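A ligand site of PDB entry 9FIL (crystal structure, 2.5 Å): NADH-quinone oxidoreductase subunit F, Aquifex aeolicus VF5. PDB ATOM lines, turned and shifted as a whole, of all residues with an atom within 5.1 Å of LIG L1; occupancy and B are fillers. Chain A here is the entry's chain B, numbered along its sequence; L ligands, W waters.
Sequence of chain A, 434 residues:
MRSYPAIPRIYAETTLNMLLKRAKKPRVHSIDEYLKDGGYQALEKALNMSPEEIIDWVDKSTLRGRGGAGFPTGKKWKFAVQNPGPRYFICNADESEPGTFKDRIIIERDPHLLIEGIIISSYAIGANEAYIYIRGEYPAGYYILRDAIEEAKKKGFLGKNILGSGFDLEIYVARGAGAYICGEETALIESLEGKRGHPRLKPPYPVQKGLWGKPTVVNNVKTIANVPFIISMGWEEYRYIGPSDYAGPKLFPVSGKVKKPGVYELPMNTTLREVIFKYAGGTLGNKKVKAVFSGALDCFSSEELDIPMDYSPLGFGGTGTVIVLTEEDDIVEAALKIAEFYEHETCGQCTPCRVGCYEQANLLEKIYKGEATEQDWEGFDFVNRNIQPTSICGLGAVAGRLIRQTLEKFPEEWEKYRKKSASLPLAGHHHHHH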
ATOM      1  N   GLY A  65       4.648  19.978 -13.199  1.00  0.00           N
ATOM      2  CA  GLY A  65       3.558  19.859 -12.251  1.00  0.00           C
ATOM      3  C   GLY A  65       2.307  20.608 -12.704  1.00  0.00           C
ATOM      4  O   GLY A  65       2.378  21.726 -13.199  1.00  0.00           O
ATOM      5  N   ARG A  66       1.155  19.966 -12.484  1.00  0.00           N
ATOM      6  CA  ARG A  66      -0.132  20.445 -12.977  1.00  0.00           C
ATOM      7  C   ARG A  66      -0.948  21.109 -11.848  1.00  0.00           C
ATOM      8  O   ARG A  66      -2.056  21.577 -12.094  1.00  0.00           O
ATOM      9  CB  ARG A  66      -0.846  19.255 -13.604  1.00  0.00           C
ATOM     10  CG  ARG A  66      -0.104  18.594 -14.757  1.00  0.00           C
ATOM     11  CD  ARG A  66      -0.227  19.322 -16.073  1.00  0.00           C
ATOM     12  NE  ARG A  66       1.027  19.268 -16.825  1.00  0.00           N
ATOM     13  CZ  ARG A  66       1.250  18.655 -17.978  1.00  0.00           C
ATOM     14  NH1 ARG A  66       2.424  18.751 -18.582  1.00  0.00           N
ATOM     15  NH2 ARG A  66       0.297  17.953 -18.559  1.00  0.00           N
ATOM     16  N   GLY A  67      -0.391  21.142 -10.634  1.00  0.00           N
ATOM     17  CA  GLY A  67      -1.041  21.809  -9.514  1.00  0.00           C
ATOM     18  C   GLY A  67      -0.838  23.319  -9.572  1.00  0.00           C
ATOM     19  O   GLY A  67      -1.371  24.039  -8.725  1.00  0.00           O
ATOM     20  N   GLY A  68      -0.003  23.757 -10.532  1.00  0.00           N
ATOM     21  CA  GLY A  68      -0.003  25.129 -11.014  1.00  0.00           C
ATOM     22  C   GLY A  68       1.331  25.869 -10.881  1.00  0.00           C
ATOM     23  O   GLY A  68       1.401  27.043 -11.272  1.00  0.00           O
ATOM     24  N   ALA A  69       2.380  25.224 -10.328  1.00  0.00           N
ATOM     25  CA  ALA A  69       3.683  25.872 -10.239  1.00  0.00           C
ATOM     26  C   ALA A  69       4.644  25.369 -11.323  1.00  0.00           C
ATOM     27  O   ALA A  69       5.657  25.988 -11.581  1.00  0.00           O
ATOM     28  CB  ALA A  69       4.247  25.685  -8.852  1.00  0.00           C
ATOM     29  N   PHE A  71       6.683  22.720 -11.644  1.00  0.00           N
ATOM     30  CA  PHE A  71       7.989  22.185 -11.304  1.00  0.00           C
ATOM     31  C   PHE A  71       8.229  20.838 -11.992  1.00  0.00           C
ATOM     32  O   PHE A  71       7.378  19.952 -11.919  1.00  0.00           O
ATOM     33  CB  PHE A  71       8.162  21.984  -9.805  1.00  0.00           C
ATOM     34  CG  PHE A  71       9.615  21.824  -9.389  1.00  0.00           C
ATOM     35  CD1 PHE A  71      10.404  22.946  -9.147  1.00  0.00           C
ATOM     36  CD2 PHE A  71      10.193  20.563  -9.241  1.00  0.00           C
ATOM     37  CE1 PHE A  71      11.734  22.807  -8.774  1.00  0.00           C
ATOM     38  CE2 PHE A  71      11.512  20.430  -8.843  1.00  0.00           C
ATOM     39  CZ  PHE A  71      12.287  21.559  -8.617  1.00  0.00           C
ATOM     40  N   LYS A  76      11.946  16.511  -9.369  1.00  0.00           N
ATOM     41  CA  LYS A  76      11.401  16.443  -8.025  1.00  0.00           C
ATOM     42  C   LYS A  76      11.656  15.063  -7.423  1.00  0.00           C
ATOM     43  O   LYS A  76      12.044  14.968  -6.264  1.00  0.00           O
ATOM     44  CB  LYS A  76       9.913  16.797  -7.977  1.00  0.00           C
ATOM     45  CG  LYS A  76       9.358  16.833  -6.561  1.00  0.00           C
ATOM     46  CD  LYS A  76       7.845  16.884  -6.435  1.00  0.00           C
ATOM     47  CE  LYS A  76       7.362  18.250  -6.728  1.00  0.00           C
ATOM     48  NZ  LYS A  76       5.901  18.366  -6.811  1.00  0.00           N
ATOM     49  N   ASN A  92      -2.037  14.841  -4.445  1.00  0.00           N
ATOM     50  CA  ASN A  92      -2.761  16.029  -4.034  1.00  0.00           C
ATOM     51  C   ASN A  92      -4.046  16.125  -4.851  1.00  0.00           C
ATOM     52  O   ASN A  92      -4.003  16.465  -6.033  1.00  0.00           O
ATOM     53  CB  ASN A  92      -1.883  17.265  -4.188  1.00  0.00           C
ATOM     54  CG  ASN A  92      -2.476  18.522  -3.596  1.00  0.00           C
ATOM     55  OD1 ASN A  92      -3.689  18.611  -3.350  1.00  0.00           O
ATOM     56  ND2 ASN A  92      -1.642  19.522  -3.390  1.00  0.00           N
ATOM     57  N   ASP A  94      -6.880  18.008  -3.688  1.00  0.00           N
ATOM     58  CA  ASP A  94      -7.648  18.948  -2.890  1.00  0.00           C
ATOM     59  C   ASP A  94      -8.518  19.872  -3.755  1.00  0.00           C
ATOM     60  O   ASP A  94      -9.484  20.424  -3.248  1.00  0.00           O
ATOM     61  CB  ASP A  94      -6.797  19.783  -1.950  1.00  0.00           C
ATOM     62  CG  ASP A  94      -7.616  20.390  -0.808  1.00  0.00           C
ATOM     63  OD1 ASP A  94      -8.105  19.597   0.031  1.00  0.00           O
ATOM     64  OD2 ASP A  94      -7.841  21.621  -0.827  1.00  0.00           O
ATOM     65  N   GLU A  95      -8.130  20.092  -5.017  1.00  0.00           N
ATOM     66  CA  GLU A  95      -8.843  20.935  -5.976  1.00  0.00           C
ATOM     67  C   GLU A  95      -9.951  21.773  -5.353  1.00  0.00           C
ATOM     68  O   GLU A  95     -11.118  21.389  -5.398  1.00  0.00           O
ATOM     69  CB  GLU A  95      -9.389  20.036  -7.083  1.00  0.00           C
ATOM     70  CG  GLU A  95      -9.844  20.841  -8.309  1.00  0.00           C
ATOM     71  CD  GLU A  95     -10.264  20.043  -9.524  1.00  0.00           C
ATOM     72  OE1 GLU A  95     -11.242  19.239  -9.424  1.00  0.00           O
ATOM     73  OE2 GLU A  95      -9.594  20.239 -10.570  1.00  0.00           O
ATOM     74  N   SER A  96      -9.600  22.972  -4.845  1.00  0.00           N
ATOM     75  CA  SER A  96     -10.558  23.861  -4.186  1.00  0.00           C
ATOM     76  C   SER A  96     -10.508  25.306  -4.681  1.00  0.00           C
ATOM     77  O   SER A  96     -11.207  26.170  -4.158  1.00  0.00           O
ATOM     78  CB  SER A  96     -10.351  23.831  -2.694  1.00  0.00           C
ATOM     79  OG  SER A  96     -10.764  22.586  -2.161  1.00  0.00           O
ATOM     80  N   ASP A 103      -9.639  17.927 -11.888  1.00  0.00           N
ATOM     81  CA  ASP A 103      -9.052  16.790 -11.191  1.00  0.00           C
ATOM     82  C   ASP A 103     -10.140  15.810 -10.799  1.00  0.00           C
ATOM     83  O   ASP A 103      -9.866  14.623 -10.651  1.00  0.00           O
ATOM     84  CB  ASP A 103      -8.245  17.248  -9.981  1.00  0.00           C
ATOM     85  CG  ASP A 103      -6.984  18.043 -10.297  1.00  0.00           C
ATOM     86  OD1 ASP A 103      -6.806  18.416 -11.492  1.00  0.00           O
ATOM     87  OD2 ASP A 103      -6.186  18.258  -9.375  1.00  0.00           O
ATOM     88  N   TYR A 180      -9.081  25.446   1.675  1.00  0.00           N
ATOM     89  CA  TYR A 180      -8.327  25.495   0.434  1.00  0.00           C
ATOM     90  C   TYR A 180      -6.824  25.431   0.711  1.00  0.00           C
ATOM     91  O   TYR A 180      -6.062  24.993  -0.152  1.00  0.00           O
ATOM     92  CB  TYR A 180      -8.798  26.759  -0.294  1.00  0.00           C
ATOM     93  CG  TYR A 180      -7.905  27.297  -1.398  1.00  0.00           C
ATOM     94  CD1 TYR A 180      -7.893  26.727  -2.661  1.00  0.00           C
ATOM     95  CD2 TYR A 180      -7.105  28.413  -1.182  1.00  0.00           C
ATOM     96  CE1 TYR A 180      -7.085  27.233  -3.667  1.00  0.00           C
ATOM     97  CE2 TYR A 180      -6.306  28.936  -2.173  1.00  0.00           C
ATOM     98  CZ  TYR A 180      -6.284  28.336  -3.423  1.00  0.00           C
ATOM     99  OH  TYR A 180      -5.511  28.818  -4.437  1.00  0.00           O
ATOM    100  N   ILE A 181      -6.402  25.885   1.907  1.00  0.00           N
ATOM    101  CA  ILE A 181      -4.991  25.902   2.274  1.00  0.00           C
ATOM    102  C   ILE A 181      -4.434  24.475   2.305  1.00  0.00           C
ATOM    103  O   ILE A 181      -3.269  24.282   2.003  1.00  0.00           O
ATOM    104  CB  ILE A 181      -4.785  26.660   3.604  1.00  0.00           C
ATOM    105  CG1 ILE A 181      -3.343  27.145   3.758  1.00  0.00           C
ATOM    106  CG2 ILE A 181      -5.226  25.833   4.822  1.00  0.00           C
ATOM    107  CD1 ILE A 181      -2.807  27.893   2.562  1.00  0.00           C
ATOM    108  N   GLY A 183      -4.618  22.407   0.269  1.00  0.00           N
ATOM    109  CA  GLY A 183      -4.128  22.043  -1.048  1.00  0.00           C
ATOM    110  C   GLY A 183      -2.673  22.458  -1.259  1.00  0.00           C
ATOM    111  O   GLY A 183      -1.993  21.943  -2.137  1.00  0.00           O
ATOM    112  N   GLU A 184      -2.243  23.465  -0.484  1.00  0.00           N
ATOM    113  CA  GLU A 184      -0.823  23.801  -0.420  1.00  0.00           C
ATOM    114  C   GLU A 184      -0.123  22.584   0.180  1.00  0.00           C
ATOM    115  O   GLU A 184      -0.645  22.016   1.136  1.00  0.00           O
ATOM    116  CB  GLU A 184      -0.644  25.127   0.313  1.00  0.00           C
ATOM    117  CG  GLU A 184       0.759  25.695   0.166  1.00  0.00           C
ATOM    118  CD  GLU A 184       1.795  25.126   1.120  1.00  0.00           C
ATOM    119  OE1 GLU A 184       1.357  24.526   2.112  1.00  0.00           O
ATOM    120  OE2 GLU A 184       3.017  25.294   0.889  1.00  0.00           O
ATOM    121  N   GLU A 185       0.990  22.160  -0.424  1.00  0.00           N
ATOM    122  CA  GLU A 185       1.570  20.828  -0.177  1.00  0.00           C
ATOM    123  C   GLU A 185       1.978  20.619   1.290  1.00  0.00           C
ATOM    124  O   GLU A 185       1.737  19.544   1.820  1.00  0.00           O
ATOM    125  CB  GLU A 185       2.716  20.545  -1.146  1.00  0.00           C
ATOM    126  CG  GLU A 185       3.904  21.477  -0.959  1.00  0.00           C
ATOM    127  CD  GLU A 185       5.130  21.263  -1.831  1.00  0.00           C
ATOM    128  OE1 GLU A 185       5.285  20.199  -2.489  1.00  0.00           O
ATOM    129  OE2 GLU A 185       5.963  22.203  -1.824  1.00  0.00           O
ATOM    130  N   VAL A 218       4.943  15.260  -3.176  1.00  0.00           N
ATOM    131  CA  VAL A 218       3.565  15.634  -3.394  1.00  0.00           C
ATOM    132  C   VAL A 218       3.413  15.967  -4.871  1.00  0.00           C
ATOM    133  O   VAL A 218       4.176  16.787  -5.385  1.00  0.00           O
ATOM    134  CB  VAL A 218       3.138  16.827  -2.499  1.00  0.00           C
ATOM    135  CG1 VAL A 218       1.687  17.217  -2.769  1.00  0.00           C
ATOM    136  CG2 VAL A 218       3.351  16.507  -1.023  1.00  0.00           C
ATOM    137  N   ASN A 219       2.520  15.242  -5.548  1.00  0.00           N
ATOM    138  CA  ASN A 219       2.173  15.528  -6.923  1.00  0.00           C
ATOM    139  C   ASN A 219       0.659  15.648  -7.038  1.00  0.00           C
ATOM    140  O   ASN A 219      -0.094  15.080  -6.245  1.00  0.00           O
ATOM    141  CB  ASN A 219       2.688  14.497  -7.918  1.00  0.00           C
ATOM    142  CG  ASN A 219       4.100  14.782  -8.391  1.00  0.00           C
ATOM    143  OD1 ASN A 219       4.370  15.862  -8.933  1.00  0.00           O
ATOM    144  ND2 ASN A 219       4.991  13.812  -8.233  1.00  0.00           N
ATOM    145  N   ASN A 220       0.226  16.398  -8.057  1.00  0.00           N
ATOM    146  CA  ASN A 220      -1.175  16.701  -8.298  1.00  0.00           C
ATOM    147  C   ASN A 220      -1.770  15.513  -9.049  1.00  0.00           C
ATOM    148  O   ASN A 220      -1.055  14.800  -9.741  1.00  0.00           O
ATOM    149  CB  ASN A 220      -1.284  18.017  -9.066  1.00  0.00           C
ATOM    150  CG  ASN A 220      -2.699  18.247  -9.548  1.00  0.00           C
ATOM    151  OD1 ASN A 220      -3.574  18.675  -8.786  1.00  0.00           O
ATOM    152  ND2 ASN A 220      -2.946  17.939 -10.809  1.00  0.00           N
ATOM    153  N   VAL A 221      -3.093  15.329  -8.945  1.00  0.00           N
ATOM    154  CA  VAL A 221      -3.805  14.235  -9.597  1.00  0.00           C
ATOM    155  C   VAL A 221      -3.411  14.111 -11.066  1.00  0.00           C
ATOM    156  O   VAL A 221      -3.010  13.058 -11.518  1.00  0.00           O
ATOM    157  CB  VAL A 221      -5.311  14.447  -9.431  1.00  0.00           C
ATOM    158  CG1 VAL A 221      -6.120  13.587 -10.401  1.00  0.00           C
ATOM    159  CG2 VAL A 221      -5.754  14.198  -7.995  1.00  0.00           C
ATOM    160  N   THR A 223      -0.878  15.379 -12.719  1.00  0.00           N
ATOM    161  CA  THR A 223       0.538  15.115 -12.965  1.00  0.00           C
ATOM    162  C   THR A 223       0.751  13.595 -13.001  1.00  0.00           C
ATOM    163  O   THR A 223       1.307  13.067 -13.945  1.00  0.00           O
ATOM    164  CB  THR A 223       1.471  15.728 -11.916  1.00  0.00           C
ATOM    165  OG1 THR A 223       1.171  17.120 -11.756  1.00  0.00           O
ATOM    166  CG2 THR A 223       2.932  15.527 -12.294  1.00  0.00           C
ATOM    167  N   CYS A 393       3.387  31.142   2.608  1.00  0.00           N
ATOM    168  CA  CYS A 393       2.899  30.379   1.450  1.00  0.00           C
ATOM    169  C   CYS A 393       2.373  31.334   0.384  1.00  0.00           C
ATOM    170  O   CYS A 393       2.430  32.554   0.553  1.00  0.00           O
ATOM    171  CB  CYS A 393       1.873  29.300   1.792  1.00  0.00           C
ATOM    172  SG  CYS A 393       0.153  29.862   1.860  1.00  0.00           S
ATOM    173  N   GLY A 394       1.886  30.735  -0.722  1.00  0.00           N
ATOM    174  CA  GLY A 394       1.556  31.439  -1.955  1.00  0.00           C
ATOM    175  C   GLY A 394       0.197  32.129  -1.931  1.00  0.00           C
ATOM    176  O   GLY A 394      -0.041  33.031  -2.740  1.00  0.00           O
ATOM    177  N   LEU A 395      -0.674  31.735  -0.990  1.00  0.00           N
ATOM    178  CA  LEU A 395      -1.951  32.388  -0.795  1.00  0.00           C
ATOM    179  C   LEU A 395      -1.746  33.887  -0.556  1.00  0.00           C
ATOM    180  O   LEU A 395      -2.254  34.718  -1.304  1.00  0.00           O
ATOM    181  CB  LEU A 395      -2.751  31.752   0.352  1.00  0.00           C
ATOM    182  CG  LEU A 395      -4.228  32.147   0.442  1.00  0.00           C
ATOM    183  CD1 LEU A 395      -5.069  31.003   0.969  1.00  0.00           C
ATOM    184  CD2 LEU A 395      -4.481  33.388   1.312  1.00  0.00           C
HETATM  185  C1  LIG L   1      -1.648  24.777  -3.991  1.00  0.00           C
HETATM  186  N1  LIG L   1      -1.279  23.653  -4.794  1.00  0.00           N
HETATM  187  C2  LIG L   1      -2.266  22.753  -5.156  1.00  0.00           C
HETATM  188  N2  LIG L   1      -1.911  21.630  -5.871  1.00  0.00           N
HETATM  189  C3  LIG L   1      -2.789  20.620  -6.141  1.00  0.00           C
HETATM  190  O1  LIG L   1      -2.441  19.571  -6.625  1.00  0.00           O
HETATM  191  N3  LIG L   1      -4.074  20.835  -5.770  1.00  0.00           N
HETATM  192  C4  LIG L   1      -4.562  21.932  -5.105  1.00  0.00           C
HETATM  193  O2  LIG L   1      -5.751  21.989  -4.849  1.00  0.00           O
HETATM  194  C5  LIG L   1      -3.578  22.907  -4.789  1.00  0.00           C
HETATM  195  N4  LIG L   1      -3.933  23.990  -4.064  1.00  0.00           N
HETATM  196  C6  LIG L   1      -2.992  24.923  -3.634  1.00  0.00           C
HETATM  197  C7  LIG L   1      -3.384  26.012  -2.848  1.00  0.00           C
HETATM  198  C8  LIG L   1      -2.456  26.950  -2.434  1.00  0.00           C
HETATM  199  C9  LIG L   1      -2.941  28.165  -1.673  1.00  0.00           C
HETATM  200  C10 LIG L   1      -1.111  26.811  -2.784  1.00  0.00           C
HETATM  201  C11 LIG L   1      -0.074  27.821  -2.358  1.00  0.00           C
HETATM  202  C12 LIG L   1      -0.713  25.716  -3.566  1.00  0.00           C
HETATM  203  C13 LIG L   1       0.116  23.468  -5.213  1.00  0.00           C
HETATM  204  C14 LIG L   1       0.898  22.649  -4.183  1.00  0.00           C
HETATM  205  O3  LIG L   1       1.541  23.532  -3.260  1.00  0.00           O
HETATM  206  C15 LIG L   1       1.951  21.797  -4.906  1.00  0.00           C
HETATM  207  O4  LIG L   1       2.590  22.519  -5.947  1.00  0.00           O
HETATM  208  C16 LIG L   1       1.379  20.513  -5.510  1.00  0.00           C
HETATM  209  O5  LIG L   1       0.737  19.750  -4.500  1.00  0.00           O
HETATM  210  C17 LIG L   1       2.448  19.678  -6.183  1.00  0.00           C
HETATM  211  O6  LIG L   1       1.930  19.595  -7.502  1.00  0.00           O
HETATM  212  P1  LIG L   1       2.723  19.120  -8.826  1.00  0.00           P
HETATM  213  O7  LIG L   1       2.283  17.691  -8.923  1.00  0.00           O
HETATM  214  O8  LIG L   1       4.219  19.316  -8.731  1.00  0.00           O
HETATM  215  O9  LIG L   1       2.091  20.032  -9.847  1.00  0.00           O
HETATM  216  P1  LG2 L   2       6.501  26.348  -5.518  1.00  0.00           P
HETATM  217  O1  LG2 L   2       7.170  26.928  -6.715  1.00  0.00           O
HETATM  218  O2  LG2 L   2       6.989  26.821  -4.188  1.00  0.00           O
HETATM  219  O3  LG2 L   2       6.671  24.763  -5.564  1.00  0.00           O
HETATM  220  C1  LG2 L   2       6.044  23.966  -6.591  1.00  0.00           C
HETATM  221  C2  LG2 L   2       6.386  22.509  -6.383  1.00  0.00           C
HETATM  222  O4  LG2 L   2       7.786  22.306  -6.699  1.00  0.00           O
HETATM  223  C3  LG2 L   2       6.249  21.983  -4.947  1.00  0.00           C
HETATM  224  O5  LG2 L   2       6.008  20.588  -4.920  1.00  0.00           O
HETATM  225  C4  LG2 L   2       7.627  22.283  -4.376  1.00  0.00           C
HETATM  226  O6  LG2 L   2       8.002  21.550  -3.228  1.00  0.00           O
HETATM  227  C5  LG2 L   2       8.502  21.898  -5.553  1.00  0.00           C
HETATM  228  N1  LG2 L   2       9.816  22.552  -5.516  1.00  0.00           N
HETATM  229  C6  LG2 L   2      10.095  23.849  -5.874  1.00  0.00           C
HETATM  230  N2  LG2 L   2      11.352  24.166  -5.716  1.00  0.00           N
HETATM  231  C7  LG2 L   2      11.936  23.002  -5.235  1.00  0.00           C
HETATM  232  C8  LG2 L   2      13.262  22.708  -4.894  1.00  0.00           C
HETATM  233  N3  LG2 L   2      14.252  23.576  -4.990  1.00  0.00           N
HETATM  234  N4  LG2 L   2      13.516  21.462  -4.439  1.00  0.00           N
HETATM  235  C9  LG2 L   2      12.495  20.593  -4.348  1.00  0.00           C
HETATM  236  N5  LG2 L   2      11.213  20.756  -4.643  1.00  0.00           N
HETATM  237  C10 LG2 L   2      10.991  22.010  -5.087  1.00  0.00           C
HETATM  238  O7  LG2 L   2       4.910  26.532  -5.588  1.00  0.00           O
HETATM  239  P2  LG2 L   2       3.710  26.159  -4.573  1.00  0.00           P
HETATM  240  O8  LG2 L   2       3.671  27.111  -3.407  1.00  0.00           O
HETATM  241  O9  LG2 L   2       3.793  24.704  -4.262  1.00  0.00           O
HETATM  242  O10 LG2 L   2       2.394  26.430  -5.482  1.00  0.00           O
HETATM  243  C11 LG2 L   2       1.923  27.786  -5.783  1.00  0.00           C
HETATM  244  C12 LG2 L   2       0.956  27.782  -6.952  1.00  0.00           C
HETATM  245  O11 LG2 L   2       0.145  26.580  -6.936  1.00  0.00           O
HETATM  246  C13 LG2 L   2      -0.101  28.905  -6.968  1.00  0.00           C
HETATM  247  O12 LG2 L   2       0.427  30.150  -7.419  1.00  0.00           O
HETATM  248  C14 LG2 L   2      -1.177  28.331  -7.914  1.00  0.00           C
HETATM  249  O13 LG2 L   2      -0.904  28.470  -9.308  1.00  0.00           O
HETATM  250  C15 LG2 L   2      -1.148  26.845  -7.501  1.00  0.00           C
HETATM  251  N6  LG2 L   2      -2.184  26.469  -6.501  1.00  0.00           N
HETATM  252  O   HOH W   1       4.970  22.012  -9.375  1.00  0.00           O
HETATM  253  O   HOH W   2      -5.818  18.756  -6.614  1.00  0.00           O
HETATM  254  O   HOH W   3       2.332  22.746  -8.869  1.00  0.00           O
HETATM  255  O   HOH W   4      -6.912  23.505  -2.684  1.00  0.00           O
HETATM  256  O   HOH W   5       6.102  17.833 -10.419  1.00  0.00           O
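The backbone NH of Asn 220 sits at hydrogen-bond distance from an oxygen (O7) of LIG L1, 2.6 Å away.
OD1 of Asn 220 lies close to O1 of LIG L1, at 2.6 Å.
The side-chain amide nitrogen (ND2) of Asn 92 lies within hydrogen-bond range of an oxygen (O5) of LIG L1 (2.6 Å).
NZ of Lys 76 lies within salt-bridge range of O8 of LIG L1, 2.7 Å away.
OD1 of Asn 219 sits close to O7 of LIG L1 (2.8 Å).
An oxygen (O9) of LIG L1 is in hydrogen-bond range of the backbone NH of Arg 66, 2.8 Å away.
The backbone NH (N) of Gly 67 lies within hydrogen-bond range of an oxygen (O9) of LIG L1, 2.8 Å away.
An oxygen (O2) of LIG L1 sits at hydrogen-bond distance from the backbone NH (N) of Glu 95, 3.0 Å away.
OG1 of Thr 223 is in hydrogen-bond range of O7 of LIG L1.
The backbone carbonyl oxygen of Gly 183 sits close to a nitrogen (N4) of LIG L1, at 3.4 Å.
The backbone NH (N) of Glu 185 is in hydrogen-bond range of an oxygen (O3) of LIG L1 (3.2 Å).
The side-chain amino group (NZ) of Lys 76 is in hydrogen-bond range of an oxygen (O5) of LG2 L2, 2.9 Å away.
O6 of LG2 L2 sits at hydrogen-bond distance from OE2 of Glu 185.
O of Gly 68 is in hydrogen-bond range of O13 of LG2 L2, 3.3 Å away.
O9 of LG2 L2 lies within hydrogen-bond range of O3 of LIG L1 (2.7 Å).
OD1 of Asn 220 sits close to OD2 of Asp 103, at 2.7 Å.
N of Asn 92 sits at hydrogen-bond distance from O of Asn 219 (2.7 Å).
O of Gly 183 lies within hydrogen-bond range of ND2 of Asn 92.
N of Asp 94 lies within hydrogen-bond range of OD1 of Asn 92 (3.3 Å).
NZ of Lys 76 sits at hydrogen-bond distance from O of Val 218.
N of Gly 65 sits at hydrogen-bond distance from O of Phe 71.
N of Asp 103 sits at hydrogen-bond distance from OE2 of Glu 95 (2.7 Å).
The side-chain carboxylate (OD2) of Asp 94 sits at hydrogen-bond distance from the backbone NH (N) of Gly 183 (3.5 Å).
Gly 65 touches LIG L1 (CA to O9, 2.8 Å).
Asp 94 touches LIG L1.
Ser 96 touches LIG L1 (N to O2, 3.97 Å).
CE2 of Tyr 180 touches C9 of LIG L1 (3.5 Å).
CG of Glu 184 touches C11 of LIG L1, 3.4 Å away.
Val 218 touches LIG L1 (CG1 to O5, 3.2 Å).
Gly 394 touches LIG L1.
Hydrophobic or aromatic side chains within 4 Å of LIG L1: Tyr 180 and Val 218.
17 residues have an atom within 4 Å of LIG L1: Gly 65, Arg 66, Gly 67, Lys 76, Asn 92, Asp 94, Glu 95, Ser 96, Tyr 180, Gly 183, Glu 184, Glu 185, Val 218, Asn 219, Asn 220, Thr 223 and Gly 394.
Along chain A the residues within 4 Å of LIG L1 span positions 65 to 394.
Water W1 lies within hydrogen-bond range of an oxygen (O8) of LIG L1 (2.9 Å) and the backbone NH (N) of Phe 71 (2.9 Å).
Water W3 lies within hydrogen-bond range of N of Ala 69, O9 of LIG L1 and N of Gly 68.
Water W5 lies within hydrogen-bond range of O of Phe 71 (2.9 Å), O8 of LIG L1 (2.9 Å) and OD1 of Asn 219 (3.0 Å).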
